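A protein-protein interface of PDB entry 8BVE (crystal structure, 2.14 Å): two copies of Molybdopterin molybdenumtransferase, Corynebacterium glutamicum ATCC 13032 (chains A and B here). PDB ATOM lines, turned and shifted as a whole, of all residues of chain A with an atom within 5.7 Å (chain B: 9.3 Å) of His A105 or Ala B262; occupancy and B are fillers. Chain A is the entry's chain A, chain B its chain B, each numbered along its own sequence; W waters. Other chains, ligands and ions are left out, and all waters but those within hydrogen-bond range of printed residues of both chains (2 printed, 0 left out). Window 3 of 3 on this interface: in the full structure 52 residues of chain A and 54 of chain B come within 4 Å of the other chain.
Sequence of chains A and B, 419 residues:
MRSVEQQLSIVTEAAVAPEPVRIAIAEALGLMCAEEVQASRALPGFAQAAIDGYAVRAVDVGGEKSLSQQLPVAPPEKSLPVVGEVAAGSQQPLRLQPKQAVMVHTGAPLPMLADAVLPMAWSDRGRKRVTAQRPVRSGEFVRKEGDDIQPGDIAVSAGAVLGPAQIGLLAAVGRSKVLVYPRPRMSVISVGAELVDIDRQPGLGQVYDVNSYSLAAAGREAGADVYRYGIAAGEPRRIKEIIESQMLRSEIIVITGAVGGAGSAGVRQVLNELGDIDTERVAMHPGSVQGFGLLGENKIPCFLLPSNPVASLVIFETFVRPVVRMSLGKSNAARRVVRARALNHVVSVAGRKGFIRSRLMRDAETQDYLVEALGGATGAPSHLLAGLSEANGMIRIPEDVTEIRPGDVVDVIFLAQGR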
ATOM      1  N   ALA A  49     -15.134 -32.002  34.027  1.00  0.00           N
ATOM      2  CA  ALA A  49     -14.939 -30.561  34.006  1.00  0.00           C
ATOM      3  C   ALA A  49     -16.285 -29.851  34.048  1.00  0.00           C
ATOM      4  O   ALA A  49     -17.212 -30.206  33.314  1.00  0.00           O
ATOM      5  CB  ALA A  49     -14.163 -30.148  32.757  1.00  0.00           C
ATOM      6  N   ILE A  51     -16.517 -26.603  33.397  1.00  0.00           N
ATOM      7  CA  ILE A  51     -16.398 -25.444  32.519  1.00  0.00           C
ATOM      8  C   ILE A  51     -15.355 -25.763  31.454  1.00  0.00           C
ATOM      9  O   ILE A  51     -14.570 -26.706  31.588  1.00  0.00           O
ATOM     10  CB  ILE A  51     -16.004 -24.177  33.327  1.00  0.00           C
ATOM     11  CG1 ILE A  51     -16.216 -22.895  32.521  1.00  0.00           C
ATOM     12  CG2 ILE A  51     -14.556 -24.267  33.808  1.00  0.00           C
ATOM     13  CD1 ILE A  51     -16.024 -21.631  33.334  1.00  0.00           C
ATOM     14  N   ASP A  52     -15.348 -24.966  30.385  1.00  0.00           N
ATOM     15  CA  ASP A  52     -14.258 -25.010  29.419  1.00  0.00           C
ATOM     16  C   ASP A  52     -12.988 -24.483  30.078  1.00  0.00           C
ATOM     17  O   ASP A  52     -13.018 -23.458  30.765  1.00  0.00           O
ATOM     18  CB  ASP A  52     -14.586 -24.161  28.186  1.00  0.00           C
ATOM     19  CG  ASP A  52     -15.533 -24.856  27.206  1.00  0.00           C
ATOM     20  OD1 ASP A  52     -16.219 -25.828  27.588  1.00  0.00           O
ATOM     21  OD2 ASP A  52     -15.594 -24.412  26.042  1.00  0.00           O
ATOM     22  N   GLY A  53     -11.875 -25.184  29.884  1.00  0.00           N
ATOM     23  CA  GLY A  53     -10.623 -24.709  30.455  1.00  0.00           C
ATOM     24  C   GLY A  53      -9.526 -25.745  30.362  1.00  0.00           C
ATOM     25  O   GLY A  53      -9.474 -26.536  29.413  1.00  0.00           O
ATOM     26  N   GLU A  85      -6.448 -32.370  24.419  1.00  0.00           N
ATOM     27  CA  GLU A  85      -7.751 -31.724  24.483  1.00  0.00           C
ATOM     28  C   GLU A  85      -8.821 -32.801  24.566  1.00  0.00           C
ATOM     29  O   GLU A  85      -8.826 -33.735  23.759  1.00  0.00           O
ATOM     30  CB  GLU A  85      -7.985 -30.824  23.263  1.00  0.00           C
ATOM     31  CG  GLU A  85      -9.446 -30.484  23.007  1.00  0.00           C
ATOM     32  CD  GLU A  85      -9.641 -29.637  21.762  1.00  0.00           C
ATOM     33  OE1 GLU A  85      -8.729 -29.609  20.907  1.00  0.00           O
ATOM     34  OE2 GLU A  85     -10.711 -29.003  21.635  1.00  0.00           O
ATOM     35  N   VAL A  86      -9.714 -32.675  25.545  1.00  0.00           N
ATOM     36  CA  VAL A  86     -10.753 -33.663  25.812  1.00  0.00           C
ATOM     37  C   VAL A  86     -12.106 -32.982  25.670  1.00  0.00           C
ATOM     38  O   VAL A  86     -12.370 -31.971  26.329  1.00  0.00           O
ATOM     39  CB  VAL A  86     -10.602 -34.290  27.211  1.00  0.00           C
ATOM     40  CG1 VAL A  86     -11.706 -35.308  27.462  1.00  0.00           C
ATOM     41  CG2 VAL A  86      -9.234 -34.936  27.363  1.00  0.00           C
ATOM     42  N   ALA A  87     -12.966 -33.546  24.829  1.00  0.00           N
ATOM     43  CA  ALA A  87     -14.315 -33.037  24.643  1.00  0.00           C
ATOM     44  C   ALA A  87     -15.318 -33.885  25.410  1.00  0.00           C
ATOM     45  O   ALA A  87     -15.028 -35.007  25.835  1.00  0.00           O
ATOM     46  CB  ALA A  87     -14.688 -33.013  23.157  1.00  0.00           C
ATOM     47  N   ALA A  88     -16.511 -33.320  25.593  1.00  0.00           N
ATOM     48  CA  ALA A  88     -17.593 -34.050  26.234  1.00  0.00           C
ATOM     49  C   ALA A  88     -17.894 -35.323  25.457  1.00  0.00           C
ATOM     50  O   ALA A  88     -17.892 -35.331  24.223  1.00  0.00           O
ATOM     51  CB  ALA A  88     -18.845 -33.173  26.335  1.00  0.00           C
ATOM     52  N   MET A 103      -6.530 -29.389  27.827  1.00  0.00           N
ATOM     53  CA  MET A 103      -7.749 -28.634  27.565  1.00  0.00           C
ATOM     54  C   MET A 103      -8.963 -29.539  27.702  1.00  0.00           C
ATOM     55  O   MET A 103      -8.960 -30.686  27.244  1.00  0.00           O
ATOM     56  CB  MET A 103      -7.707 -28.020  26.165  1.00  0.00           C
ATOM     57  CG  MET A 103      -6.586 -27.010  25.965  1.00  0.00           C
ATOM     58  SD  MET A 103      -6.893 -25.857  24.613  1.00  0.00           S
ATOM     59  CE  MET A 103      -6.528 -26.887  23.192  1.00  0.00           C
ATOM     60  N   VAL A 104     -10.006 -29.022  28.346  1.00  0.00           N
ATOM     61  CA  VAL A 104     -11.227 -29.782  28.573  1.00  0.00           C
ATOM     62  C   VAL A 104     -12.423 -28.924  28.195  1.00  0.00           C
ATOM     63  O   VAL A 104     -12.415 -27.698  28.360  1.00  0.00           O
ATOM     64  CB  VAL A 104     -11.349 -30.265  30.036  1.00  0.00           C
ATOM     65  CG1 VAL A 104     -10.363 -31.403  30.313  1.00  0.00           C
ATOM     66  CG2 VAL A 104     -11.126 -29.108  31.004  1.00  0.00           C
ATOM     67  N   HIS A 105     -13.454 -29.577  27.670  1.00  0.00           N
ATOM     68  CA  HIS A 105     -14.742 -28.941  27.454  1.00  0.00           C
ATOM     69  C   HIS A 105     -15.651 -29.246  28.633  1.00  0.00           C
ATOM     70  O   HIS A 105     -15.466 -30.237  29.342  1.00  0.00           O
ATOM     71  CB  HIS A 105     -15.405 -29.444  26.167  1.00  0.00           C
ATOM     72  CG  HIS A 105     -14.658 -29.099  24.918  1.00  0.00           C
ATOM     73  ND1 HIS A 105     -15.111 -29.452  23.665  1.00  0.00           N
ATOM     74  CD2 HIS A 105     -13.494 -28.438  24.725  1.00  0.00           C
ATOM     75  CE1 HIS A 105     -14.257 -29.022  22.753  1.00  0.00           C
ATOM     76  NE2 HIS A 105     -13.266 -28.406  23.370  1.00  0.00           N
ATOM     77  N   THR A 106     -16.645 -28.381  28.831  1.00  0.00           N
ATOM     78  CA  THR A 106     -17.643 -28.616  29.866  1.00  0.00           C
ATOM     79  C   THR A 106     -18.230 -30.012  29.708  1.00  0.00           C
ATOM     80  O   THR A 106     -18.633 -30.406  28.611  1.00  0.00           O
ATOM     81  CB  THR A 106     -18.761 -27.572  29.786  1.00  0.00           C
ATOM     82  OG1 THR A 106     -18.196 -26.262  29.639  1.00  0.00           O
ATOM     83  CG2 THR A 106     -19.626 -27.621  31.042  1.00  0.00           C
ATOM     84  N   GLY A 107     -18.245 -30.770  30.803  1.00  0.00           N
ATOM     85  CA  GLY A 107     -18.759 -32.121  30.796  1.00  0.00           C
ATOM     86  C   GLY A 107     -17.761 -33.191  30.406  1.00  0.00           C
ATOM     87  O   GLY A 107     -18.078 -34.382  30.530  1.00  0.00           O
ATOM     88  N   ALA A 108     -16.574 -32.812  29.936  1.00  0.00           N
ATOM     89  CA  ALA A 108     -15.576 -33.796  29.555  1.00  0.00           C
ATOM     90  C   ALA A 108     -15.060 -34.536  30.789  1.00  0.00           C
ATOM     91  O   ALA A 108     -14.994 -33.967  31.882  1.00  0.00           O
ATOM     92  CB  ALA A 108     -14.409 -33.130  28.831  1.00  0.00           C
ATOM     93  N   ALA B 193     -22.614 -34.977  22.758  1.00  0.00           N
ATOM     94  CA  ALA B 193     -22.012 -36.290  22.542  1.00  0.00           C
ATOM     95  C   ALA B 193     -21.981 -37.135  23.811  1.00  0.00           C
ATOM     96  O   ALA B 193     -21.830 -38.359  23.724  1.00  0.00           O
ATOM     97  CB  ALA B 193     -20.591 -36.141  21.986  1.00  0.00           C
ATOM     98  N   GLU B 194     -22.094 -36.514  24.983  1.00  0.00           N
ATOM     99  CA  GLU B 194     -22.051 -37.252  26.236  1.00  0.00           C
ATOM    100  C   GLU B 194     -23.364 -37.952  26.561  1.00  0.00           C
ATOM    101  O   GLU B 194     -23.378 -38.823  27.437  1.00  0.00           O
ATOM    102  CB  GLU B 194     -21.685 -36.301  27.380  1.00  0.00           C
ATOM    103  CG  GLU B 194     -22.864 -35.474  27.890  1.00  0.00           C
ATOM    104  CD  GLU B 194     -23.047 -34.153  27.146  1.00  0.00           C
ATOM    105  OE1 GLU B 194     -22.385 -33.933  26.106  1.00  0.00           O
ATOM    106  OE2 GLU B 194     -23.864 -33.329  27.603  1.00  0.00           O
ATOM    107  N   GLY B 257     -28.005 -28.116  25.845  1.00  0.00           N
ATOM    108  CA  GLY B 257     -26.680 -28.455  25.377  1.00  0.00           C
ATOM    109  C   GLY B 257     -26.161 -27.607  24.238  1.00  0.00           C
ATOM    110  O   GLY B 257     -25.061 -27.880  23.740  1.00  0.00           O
ATOM    111  N   ALA B 258     -26.901 -26.580  23.821  1.00  0.00           N
ATOM    112  CA  ALA B 258     -26.464 -25.694  22.749  1.00  0.00           C
ATOM    113  C   ALA B 258     -25.699 -24.477  23.254  1.00  0.00           C
ATOM    114  O   ALA B 258     -25.180 -23.709  22.437  1.00  0.00           O
ATOM    115  CB  ALA B 258     -27.668 -25.237  21.919  1.00  0.00           C
ATOM    116  N   VAL B 259     -25.617 -24.282  24.569  1.00  0.00           N
ATOM    117  CA  VAL B 259     -24.798 -23.235  25.168  1.00  0.00           C
ATOM    118  C   VAL B 259     -23.929 -23.867  26.246  1.00  0.00           C
ATOM    119  O   VAL B 259     -24.288 -24.885  26.848  1.00  0.00           O
ATOM    120  CB  VAL B 259     -25.643 -22.082  25.761  1.00  0.00           C
ATOM    121  CG1 VAL B 259     -26.342 -21.307  24.656  1.00  0.00           C
ATOM    122  CG2 VAL B 259     -26.657 -22.618  26.765  1.00  0.00           C
ATOM    123  N   GLY B 260     -22.764 -23.271  26.472  1.00  0.00           N
ATOM    124  CA  GLY B 260     -21.841 -23.800  27.452  1.00  0.00           C
ATOM    125  C   GLY B 260     -20.392 -23.562  27.087  1.00  0.00           C
ATOM    126  O   GLY B 260     -19.592 -23.159  27.938  1.00  0.00           O
ATOM    127  N   GLY B 261     -20.037 -23.821  25.833  1.00  0.00           N
ATOM    128  CA  GLY B 261     -18.662 -23.607  25.410  1.00  0.00           C
ATOM    129  C   GLY B 261     -18.413 -24.148  24.021  1.00  0.00           C
ATOM    130  O   GLY B 261     -19.334 -24.256  23.203  1.00  0.00           O
ATOM    131  N   ALA B 262     -17.149 -24.506  23.775  1.00  0.00           N
ATOM    132  CA  ALA B 262     -16.730 -24.950  22.449  1.00  0.00           C
ATOM    133  C   ALA B 262     -17.417 -26.244  22.029  1.00  0.00           C
ATOM    134  O   ALA B 262     -17.553 -26.507  20.830  1.00  0.00           O
ATOM    135  CB  ALA B 262     -15.212 -25.128  22.418  1.00  0.00           C
ATOM    136  N   GLY B 263     -17.852 -27.061  22.990  1.00  0.00           N
ATOM    137  CA  GLY B 263     -18.492 -28.323  22.659  1.00  0.00           C
ATOM    138  C   GLY B 263     -19.765 -28.178  21.852  1.00  0.00           C
ATOM    139  O   GLY B 263     -20.187 -29.136  21.194  1.00  0.00           O
ATOM    140  N   SER B 264     -20.387 -27.000  21.876  1.00  0.00           N
ATOM    141  CA  SER B 264     -21.631 -26.762  21.156  1.00  0.00           C
ATOM    142  C   SER B 264     -21.435 -25.801  19.991  1.00  0.00           C
ATOM    143  O   SER B 264     -22.408 -25.230  19.490  1.00  0.00           O
ATOM    144  CB  SER B 264     -22.711 -26.241  22.105  1.00  0.00           C
ATOM    145  OG  SER B 264     -22.249 -25.140  22.862  1.00  0.00           O
ATOM    146  N   ALA B 265     -20.187 -25.600  19.555  1.00  0.00           N
ATOM    147  CA  ALA B 265     -19.930 -24.677  18.457  1.00  0.00           C
ATOM    148  C   ALA B 265     -20.576 -25.166  17.167  1.00  0.00           C
ATOM    149  O   ALA B 265     -21.072 -24.362  16.369  1.00  0.00           O
ATOM    150  CB  ALA B 265     -18.423 -24.490  18.266  1.00  0.00           C
ATOM    151  N   GLY B 266     -20.588 -26.483  16.952  1.00  0.00           N
ATOM    152  CA  GLY B 266     -21.170 -27.014  15.731  1.00  0.00           C
ATOM    153  C   GLY B 266     -22.673 -26.827  15.684  1.00  0.00           C
ATOM    154  O   GLY B 266     -23.230 -26.407  14.666  1.00  0.00           O
ATOM    155  N   VAL B 267     -23.351 -27.127  16.794  1.00  0.00           N
ATOM    156  CA  VAL B 267     -24.802 -26.986  16.828  1.00  0.00           C
ATOM    157  C   VAL B 267     -25.191 -25.519  16.733  1.00  0.00           C
ATOM    158  O   VAL B 267     -26.195 -25.169  16.100  1.00  0.00           O
ATOM    159  CB  VAL B 267     -25.370 -27.646  18.094  1.00  0.00           C
ATOM    160  CG1 VAL B 267     -26.891 -27.564  18.100  1.00  0.00           C
ATOM    161  CG2 VAL B 267     -24.898 -29.087  18.173  1.00  0.00           C
ATOM    162  N   ARG B 268     -24.404 -24.635  17.352  1.00  0.00           N
ATOM    163  CA  ARG B 268     -24.670 -23.208  17.220  1.00  0.00           C
ATOM    164  C   ARG B 268     -24.421 -22.724  15.799  1.00  0.00           C
ATOM    165  O   ARG B 268     -25.126 -21.831  15.319  1.00  0.00           O
ATOM    166  CB  ARG B 268     -23.827 -22.415  18.217  1.00  0.00           C
ATOM    167  CG  ARG B 268     -24.462 -22.324  19.603  1.00  0.00           C
ATOM    168  CD  ARG B 268     -23.745 -21.318  20.489  1.00  0.00           C
ATOM    169  NE  ARG B 268     -22.613 -21.926  21.178  1.00  0.00           N
ATOM    170  CZ  ARG B 268     -21.370 -21.923  20.716  1.00  0.00           C
ATOM    171  NH1 ARG B 268     -21.061 -21.350  19.564  1.00  0.00           N
ATOM    172  NH2 ARG B 268     -20.414 -22.516  21.424  1.00  0.00           N
ATOM    173  N   GLN B 269     -23.434 -23.305  15.110  1.00  0.00           N
ATOM    174  CA  GLN B 269     -23.213 -22.961  13.710  1.00  0.00           C
ATOM    175  C   GLN B 269     -24.429 -23.316  12.869  1.00  0.00           C
ATOM    176  O   GLN B 269     -24.855 -22.534  12.011  1.00  0.00           O
ATOM    177  CB  GLN B 269     -21.967 -23.673  13.180  1.00  0.00           C
ATOM    178  CG  GLN B 269     -21.711 -23.579  11.659  1.00  0.00           C
ATOM    179  CD  GLN B 269     -22.041 -22.234  11.002  1.00  0.00           C
ATOM    180  OE1 GLN B 269     -22.420 -22.194   9.831  1.00  0.00           O
ATOM    181  NE2 GLN B 269     -21.828 -21.132  11.725  1.00  0.00           N
HETATM  182  O   HOH W   1     -18.189 -26.789  25.634  1.00  0.00           O
HETATM  183  O   HOH W   2     -17.514 -22.993  29.557  1.00  0.00           O
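Water W2 lies within hydrogen-bond range of O of Gly B260, N of Asp A52 and OG1 of Thr A106. Water W1 lies within hydrogen-bond range of the backbone NH of Gly B263 (2.7 Å), the side-chain carboxylate of Asp A52 (2.9 Å) and the backbone NH of Ala B262 (3.1 Å).
Hydrophobic or aromatic side chains of chain A within 4 Å of the printed part of chain B: Ala A88 and His A105. Of the 15 printed residues of chain B, 6 touch a printed residue of chain A. Hydrophobic or aromatic side chains of chain B within 4 Å of the printed part of chain A: Ala B193 and Ala B262. Along chain B the printed residues that touch a printed residue of chain A span positions 193 to 263. Among the printed residues, 7 pairs touch across the chains.
Among the printed residues, pairs that only touch across the chains: Asp A52 with Gly B261 (3.2 Å), Ala A88 with Ala B193 (3.6 Å), Ala A88 with Glu B194 (3.6 Å), His A105 with Ala B262 (3.9 Å), His A105 with Gly B263 (3.7 Å) and Thr A106 with Gly B260 (3.8 Å).
N of Ala B262 sits at hydrogen-bond distance from OD2 of Asp A52 (2.8 Å).
Of chain A, only Asp A52 and His A105 come within 4 Å of Ala B262. No residue of chain B comes within 4 Å of Val A104. Ala A108 touches none of the printed residues of chain B. Of the printed residues of chain B, Ala A88 touches Ala B193 (3.6 Å) and Glu B194 (3.6 Å). Of the printed residues of chain A, Gly B261 touches Asp A52. Printed residues of chain B within 4 Å of Asp A52: Gly B261 (3.2 Å) and Ala B262 (2.8 Å). Printed residues of chain A within 4 Å of Gly B263: His A105. Printed residues of chain A within 4 Å of Glu B194: Ala A88. Val A86 touches none of the printed residues of chain B. The nearest printed residue of chain A that does not touch Gly B261 is Thr A106 (4.9 Å).
No position is printed for both chains.
The backbone NH of Thr A106 lies within hydrogen-bond range of the side-chain carboxylate of Asp A52. The side-chain carboxylate (OE2) of Glu A85 lies within hydrogen-bond range of a ring nitrogen (NE2) of His A105 (3.1 Å). The backbone carbonyl oxygen (O) of Val A86 sits at hydrogen-bond distance from the backbone NH (N) of His A105, 3.0 Å away. OG of Ser B264 sits at hydrogen-bond distance from O of Gly B261 (3.1 Å). NH2 of Arg B268 lies within hydrogen-bond range of O of Gly B261 (2.7 Å).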
